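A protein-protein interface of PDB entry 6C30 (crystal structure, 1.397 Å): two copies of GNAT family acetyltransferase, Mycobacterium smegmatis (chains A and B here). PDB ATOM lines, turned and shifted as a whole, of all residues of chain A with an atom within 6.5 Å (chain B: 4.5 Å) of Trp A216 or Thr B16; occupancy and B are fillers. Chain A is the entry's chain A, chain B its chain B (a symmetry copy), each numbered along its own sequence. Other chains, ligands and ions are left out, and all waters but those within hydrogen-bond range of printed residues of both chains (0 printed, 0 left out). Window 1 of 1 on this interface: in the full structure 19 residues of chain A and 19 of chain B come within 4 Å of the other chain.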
ATOM      1  N   GLY A  18       6.912   5.574  19.969  1.00  0.00           N
ATOM      2  CA  GLY A  18       7.480   5.617  21.306  1.00  0.00           C
ATOM      3  C   GLY A  18       8.751   6.448  21.296  1.00  0.00           C
ATOM      4  O   GLY A  18       8.937   7.277  20.411  1.00  0.00           O
ATOM      5  N   PRO A  19       9.648   6.223  22.265  1.00  0.00           N
ATOM      6  CA  PRO A  19       9.571   5.194  23.303  1.00  0.00           C
ATOM      7  C   PRO A  19       8.606   5.511  24.445  1.00  0.00           C
ATOM      8  O   PRO A  19       8.246   6.669  24.687  1.00  0.00           O
ATOM      9  CB  PRO A  19      11.007   5.129  23.825  1.00  0.00           C
ATOM     10  CG  PRO A  19      11.524   6.511  23.632  1.00  0.00           C
ATOM     11  CD  PRO A  19      10.912   6.983  22.342  1.00  0.00           C
ATOM     12  N   LEU A  20       8.196   4.453  25.132  1.00  0.00           N
ATOM     13  CA  LEU A  20       7.404   4.561  26.346  1.00  0.00           C
ATOM     14  C   LEU A  20       8.200   3.964  27.476  1.00  0.00           C
ATOM     15  O   LEU A  20       9.018   3.064  27.252  1.00  0.00           O
ATOM     16  CB  LEU A  20       6.079   3.812  26.218  1.00  0.00           C
ATOM     17  CG  LEU A  20       5.203   4.077  24.998  1.00  0.00           C
ATOM     18  CD1 LEU A  20       3.952   3.239  25.120  1.00  0.00           C
ATOM     19  CD2 LEU A  20       4.865   5.556  24.905  1.00  0.00           C
ATOM     20  N   ARG A  21       7.959   4.427  28.697  1.00  0.00           N
ATOM     21  CA  ARG A  21       8.404   3.649  29.836  1.00  0.00           C
ATOM     22  C   ARG A  21       7.166   3.044  30.479  1.00  0.00           C
ATOM     23  O   ARG A  21       6.236   3.772  30.850  1.00  0.00           O
ATOM     24  CB  ARG A  21       9.200   4.484  30.846  1.00  0.00           C
ATOM     25  CG  ARG A  21       9.678   3.627  32.009  1.00  0.00           C
ATOM     26  CD  ARG A  21      10.704   4.322  32.901  1.00  0.00           C
ATOM     27  NE  ARG A  21      12.095   4.203  32.449  1.00  0.00           N
ATOM     28  CZ  ARG A  21      12.820   3.085  32.487  1.00  0.00           C
ATOM     29  NH1 ARG A  21      12.290   1.942  32.907  1.00  0.00           N
ATOM     30  NH2 ARG A  21      14.083   3.104  32.085  1.00  0.00           N
ATOM     31  N   VAL A  22       7.159   1.716  30.565  1.00  0.00           N
ATOM     32  CA  VAL A  22       6.055   0.935  31.121  1.00  0.00           C
ATOM     33  C   VAL A  22       6.662  -0.017  32.157  1.00  0.00           C
ATOM     34  O   VAL A  22       7.879  -0.049  32.299  1.00  0.00           O
ATOM     35  CB  VAL A  22       5.291   0.179  30.009  1.00  0.00           C
ATOM     36  CG1 VAL A  22       4.580   1.163  29.088  1.00  0.00           C
ATOM     37  CG2 VAL A  22       6.231  -0.729  29.236  1.00  0.00           C
ATOM     38  N   VAL A  26      11.713   0.080  28.939  1.00  0.00           N
ATOM     39  CA  VAL A  26      11.504   0.998  27.830  1.00  0.00           C
ATOM     40  C   VAL A  26      11.048   0.204  26.607  1.00  0.00           C
ATOM     41  O   VAL A  26      11.737  -0.722  26.164  1.00  0.00           O
ATOM     42  CB  VAL A  26      12.788   1.795  27.501  1.00  0.00           C
ATOM     43  CG1 VAL A  26      12.550   2.731  26.321  1.00  0.00           C
ATOM     44  CG2 VAL A  26      13.241   2.592  28.736  1.00  0.00           C
ATOM     45  N   VAL A  27       9.876   0.539  26.080  1.00  0.00           N
ATOM     46  CA  VAL A  27       9.360  -0.154  24.902  1.00  0.00           C
ATOM     47  C   VAL A  27       9.170   0.808  23.741  1.00  0.00           C
ATOM     48  O   VAL A  27       8.836   1.974  23.929  1.00  0.00           O
ATOM     49  CB  VAL A  27       8.023  -0.864  25.188  1.00  0.00           C
ATOM     50  CG1 VAL A  27       8.215  -1.978  26.212  1.00  0.00           C
ATOM     51  CG2 VAL A  27       6.962   0.136  25.627  1.00  0.00           C
ATOM     52  N   ALA A 211       0.329   7.605  29.522  1.00  0.00           N
ATOM     53  CA  ALA A 211       1.055   7.335  30.753  1.00  0.00           C
ATOM     54  C   ALA A 211       2.490   6.919  30.447  1.00  0.00           C
ATOM     55  O   ALA A 211       3.423   7.309  31.150  1.00  0.00           O
ATOM     56  CB  ALA A 211       0.350   6.257  31.567  1.00  0.00           C
ATOM     57  N   GLY A 212       2.666   6.132  29.388  1.00  0.00           N
ATOM     58  CA  GLY A 212       3.988   5.647  29.026  1.00  0.00           C
ATOM     59  C   GLY A 212       4.895   6.768  28.556  1.00  0.00           C
ATOM     60  O   GLY A 212       6.099   6.765  28.841  1.00  0.00           O
ATOM     61  N   ARG A 213       4.324   7.723  27.828  1.00  0.00           N
ATOM     62  CA  ARG A 213       5.081   8.888  27.385  1.00  0.00           C
ATOM     63  C   ARG A 213       5.463   9.767  28.564  1.00  0.00           C
ATOM     64  O   ARG A 213       6.601  10.231  28.652  1.00  0.00           O
ATOM     65  CB  ARG A 213       4.286   9.708  26.376  1.00  0.00           C
ATOM     66  CG  ARG A 213       4.145   9.048  25.011  1.00  0.00           C
ATOM     67  CD  ARG A 213       3.185   9.786  24.105  1.00  0.00           C
ATOM     68  NE  ARG A 213       3.215   9.221  22.759  1.00  0.00           N
ATOM     69  CZ  ARG A 213       2.295   9.451  21.829  1.00  0.00           C
ATOM     70  NH1 ARG A 213       1.258  10.235  22.097  1.00  0.00           N
ATOM     71  NH2 ARG A 213       2.412   8.890  20.634  1.00  0.00           N
ATOM     72  N   ALA A 214       4.505  10.004  29.456  1.00  0.00           N
ATOM     73  CA  ALA A 214       4.755  10.832  30.633  1.00  0.00           C
ATOM     74  C   ALA A 214       5.841  10.211  31.508  1.00  0.00           C
ATOM     75  O   ALA A 214       6.721  10.912  32.014  1.00  0.00           O
ATOM     76  CB  ALA A 214       3.470  11.026  31.434  1.00  0.00           C
ATOM     77  N   GLU A 215       5.787   8.896  31.685  1.00  0.00           N
ATOM     78  CA  GLU A 215       6.775   8.214  32.503  1.00  0.00           C
ATOM     79  C   GLU A 215       8.160   8.278  31.866  1.00  0.00           C
ATOM     80  O   GLU A 215       9.163   8.492  32.557  1.00  0.00           O
ATOM     81  CB  GLU A 215       6.370   6.759  32.738  1.00  0.00           C
ATOM     82  CG  GLU A 215       7.235   6.018  33.746  1.00  0.00           C
ATOM     83  CD  GLU A 215       7.154   6.596  35.156  1.00  0.00           C
ATOM     84  OE1 GLU A 215       6.173   7.302  35.470  1.00  0.00           O
ATOM     85  OE2 GLU A 215       8.079   6.333  35.952  1.00  0.00           O
ATOM     86  N   TRP A 216       8.220   8.093  30.549  1.00  0.00           N
ATOM     87  CA  TRP A 216       9.492   8.175  29.837  1.00  0.00           C
ATOM     88  C   TRP A 216      10.127   9.552  30.019  1.00  0.00           C
ATOM     89  O   TRP A 216      11.342   9.661  30.212  1.00  0.00           O
ATOM     90  CB  TRP A 216       9.313   7.877  28.337  1.00  0.00           C
ATOM     91  CG  TRP A 216      10.637   7.665  27.643  1.00  0.00           C
ATOM     92  CD1 TRP A 216      11.264   6.467  27.426  1.00  0.00           C
ATOM     93  CD2 TRP A 216      11.508   8.676  27.112  1.00  0.00           C
ATOM     94  NE1 TRP A 216      12.470   6.670  26.798  1.00  0.00           N
ATOM     95  CE2 TRP A 216      12.642   8.017  26.590  1.00  0.00           C
ATOM     96  CE3 TRP A 216      11.439  10.069  27.029  1.00  0.00           C
ATOM     97  CZ2 TRP A 216      13.694   8.703  25.988  1.00  0.00           C
ATOM     98  CZ3 TRP A 216      12.490  10.756  26.432  1.00  0.00           C
ATOM     99  CH2 TRP A 216      13.603  10.068  25.920  1.00  0.00           C
ATOM    100  N   CYS A 217       9.303  10.596  29.968  1.00  0.00           N
ATOM    101  CA  CYS A 217       9.799  11.971  29.973  1.00  0.00           C
ATOM    102  C   CYS A 217      10.235  12.470  31.348  1.00  0.00           C
ATOM    103  O   CYS A 217      10.816  13.555  31.455  1.00  0.00           O
ATOM    104  CB  CYS A 217       8.739  12.912  29.405  1.00  0.00           C
ATOM    105  SG  CYS A 217       8.516  12.736  27.631  1.00  0.00           S
ATOM    106  N   ALA A 218       9.961  11.692  32.390  1.00  0.00           N
ATOM    107  CA  ALA A 218      10.431  12.034  33.733  1.00  0.00           C
ATOM    108  C   ALA A 218      11.958  12.006  33.770  1.00  0.00           C
ATOM    109  O   ALA A 218      12.579  10.960  33.562  1.00  0.00           O
ATOM    110  CB  ALA A 218       9.852  11.074  34.762  1.00  0.00           C
ATOM    111  N   ALA A 219      12.569  13.161  34.030  1.00  0.00           N
ATOM    112  CA  ALA A 219      14.023  13.237  34.140  1.00  0.00           C
ATOM    113  C   ALA A 219      14.491  12.678  35.480  1.00  0.00           C
ATOM    114  O   ALA A 219      13.804  12.816  36.491  1.00  0.00           O
ATOM    115  CB  ALA A 219      14.496  14.676  33.967  1.00  0.00           C
ATOM    116  N   PRO B  14      14.711  14.854  28.863  1.00  0.00           N
ATOM    117  CA  PRO B  14      15.301  13.744  28.110  1.00  0.00           C
ATOM    118  C   PRO B  14      14.759  13.720  26.687  1.00  0.00           C
ATOM    119  O   PRO B  14      13.686  14.249  26.413  1.00  0.00           O
ATOM    120  CB  PRO B  14      14.853  12.511  28.897  1.00  0.00           C
ATOM    121  CG  PRO B  14      13.551  12.920  29.503  1.00  0.00           C
ATOM    122  CD  PRO B  14      13.647  14.402  29.779  1.00  0.00           C
ATOM    123  N   ASP B  15      15.507  13.112  25.778  1.00  0.00           N
ATOM    124  CA  ASP B  15      15.071  13.010  24.398  1.00  0.00           C
ATOM    125  C   ASP B  15      15.869  11.902  23.737  1.00  0.00           C
ATOM    126  O   ASP B  15      16.841  11.402  24.313  1.00  0.00           O
ATOM    127  CB  ASP B  15      15.272  14.341  23.660  1.00  0.00           C
ATOM    128  CG  ASP B  15      14.347  14.504  22.463  1.00  0.00           C
ATOM    129  OD1 ASP B  15      13.618  13.552  22.115  1.00  0.00           O
ATOM    130  OD2 ASP B  15      14.367  15.599  21.855  1.00  0.00           O
ATOM    131  N   THR B  16      15.440  11.503  22.543  1.00  0.00           N
ATOM    132  CA  THR B  16      16.264  10.657  21.694  1.00  0.00           C
ATOM    133  C   THR B  16      16.732  11.496  20.514  1.00  0.00           C
ATOM    134  O   THR B  16      16.165  12.560  20.233  1.00  0.00           O
ATOM    135  CB  THR B  16      15.509   9.419  21.189  1.00  0.00           C
ATOM    136  OG1 THR B  16      14.425   9.836  20.353  1.00  0.00           O
ATOM    137  CG2 THR B  16      14.960   8.608  22.354  1.00  0.00           C
ATOM    138  N   VAL B  17      17.775  11.030  19.835  1.00  0.00           N
ATOM    139  CA  VAL B  17      18.265  11.700  18.634  1.00  0.00           C
ATOM    140  C   VAL B  17      18.427  10.657  17.538  1.00  0.00           C
ATOM    141  O   VAL B  17      18.846   9.524  17.796  1.00  0.00           O
ATOM    142  CB  VAL B  17      19.597  12.440  18.880  1.00  0.00           C
ATOM    143  CG1 VAL B  17      19.925  13.359  17.710  1.00  0.00           C
ATOM    144  CG2 VAL B  17      19.515  13.252  20.176  1.00  0.00           C
ATOM    145  N   GLY B  18      18.061  11.029  16.316  1.00  0.00           N
ATOM    146  CA  GLY B  18      18.064  10.067  15.233  1.00  0.00           C
ATOM    147  C   GLY B  18      16.725   9.368  15.193  1.00  0.00           C
ATOM    148  O   GLY B  18      15.730   9.912  15.662  1.00  0.00           O
ATOM    149  N   LEU B  29      20.918   8.196  19.439  1.00  0.00           N
ATOM    150  CA  LEU B  29      21.278   8.566  20.813  1.00  0.00           C
ATOM    151  C   LEU B  29      20.050   8.464  21.696  1.00  0.00           C
ATOM    152  O   LEU B  29      18.957   8.862  21.296  1.00  0.00           O
ATOM    153  CB  LEU B  29      21.820   9.994  20.891  1.00  0.00           C
ATOM    154  CG  LEU B  29      23.019  10.356  20.021  1.00  0.00           C
ATOM    155  CD1 LEU B  29      23.455  11.796  20.272  1.00  0.00           C
ATOM    156  CD2 LEU B  29      24.179   9.419  20.287  1.00  0.00           C
ATOM    157  N   ARG B  30      20.221   7.946  22.904  1.00  0.00           N
ATOM    158  CA  ARG B  30      19.118   7.948  23.862  1.00  0.00           C
ATOM    159  C   ARG B  30      19.698   8.013  25.287  1.00  0.00           C
ATOM    160  O   ARG B  30      20.885   7.767  25.492  1.00  0.00           O
ATOM    161  CB  ARG B  30      18.195   6.727  23.653  1.00  0.00           C
ATOM    162  CG  ARG B  30      18.879   5.375  23.635  1.00  0.00           C
ATOM    163  CD  ARG B  30      19.096   4.840  25.042  1.00  0.00           C
ATOM    164  NE  ARG B  30      19.701   3.510  25.021  1.00  0.00           N
ATOM    165  CZ  ARG B  30      20.297   2.958  26.070  1.00  0.00           C
ATOM    166  NH1 ARG B  30      20.359   3.614  27.223  1.00  0.00           N
ATOM    167  NH2 ARG B  30      20.835   1.754  25.972  1.00  0.00           N
ATOM    168  N   PRO B  31      18.868   8.372  26.273  1.00  0.00           N
ATOM    169  CA  PRO B  31      19.414   8.575  27.624  1.00  0.00           C
ATOM    170  C   PRO B  31      20.021   7.330  28.270  1.00  0.00           C
ATOM    171  O   PRO B  31      19.513   6.214  28.100  1.00  0.00           O
ATOM    172  CB  PRO B  31      18.186   9.036  28.419  1.00  0.00           C
ATOM    173  CG  PRO B  31      17.301   9.684  27.395  1.00  0.00           C
ATOM    174  CD  PRO B  31      17.457   8.797  26.180  1.00  0.00           C
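Among the printed residues, pairs that only touch across the chains: Trp A216 with Pro B14, Trp A216 with Asp B15, Trp A216 with Thr B16, Trp A216 with Pro B31 and Cys A217 with Pro B14.
Pro A19 touches none of the printed residues of chain B.
Trp A216 touches just these residues of chain B: Pro B14, Asp B15, Thr B16 and Pro B31.
Printed residues of chain B within 4 Å of Cys A217: Pro B14 (3.4 Å).
Printed residues of chain A within 4 Å of Thr B16: Trp A216 (3.8 Å).
Printed residues of chain A within 4 Å of Pro B31: Trp A216.
The nearest residue of chain A that does not touch Thr B16 is Pro A19 (4.2 Å).
The nearest printed residue of chain A that does not touch Pro B14 is Ala A219 (4.3 Å).
Of the 16 printed residues of chain A, 2 touch a printed residue of chain B.
Hydrophobic or aromatic side chains of chain A that line the printed part of chain B: Trp A216.
Of the 8 printed residues of chain B, 4 touch a printed residue of chain A.
Printed residues of chain B that touch a printed residue of chain A: Pro B14, Asp B15, Thr B16 and Pro B31.
Along chain B the printed residues that touch a printed residue of chain A span positions 14 to 31.
Among the printed residues, no Asp or Glu carboxylate lies within 4 Å of a Lys or Arg side-chain nitrogen of the other chain.
The backbone carbonyl oxygen (O) of Arg A213 sits at hydrogen-bond distance from the side-chain sulfur (SG) of Cys A217 (3.3 Å).
Position printed for both chains: 18.
Of the 5 pairs that touch across the chains among the printed residues, none has its exchanged pair printed and touching as well.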
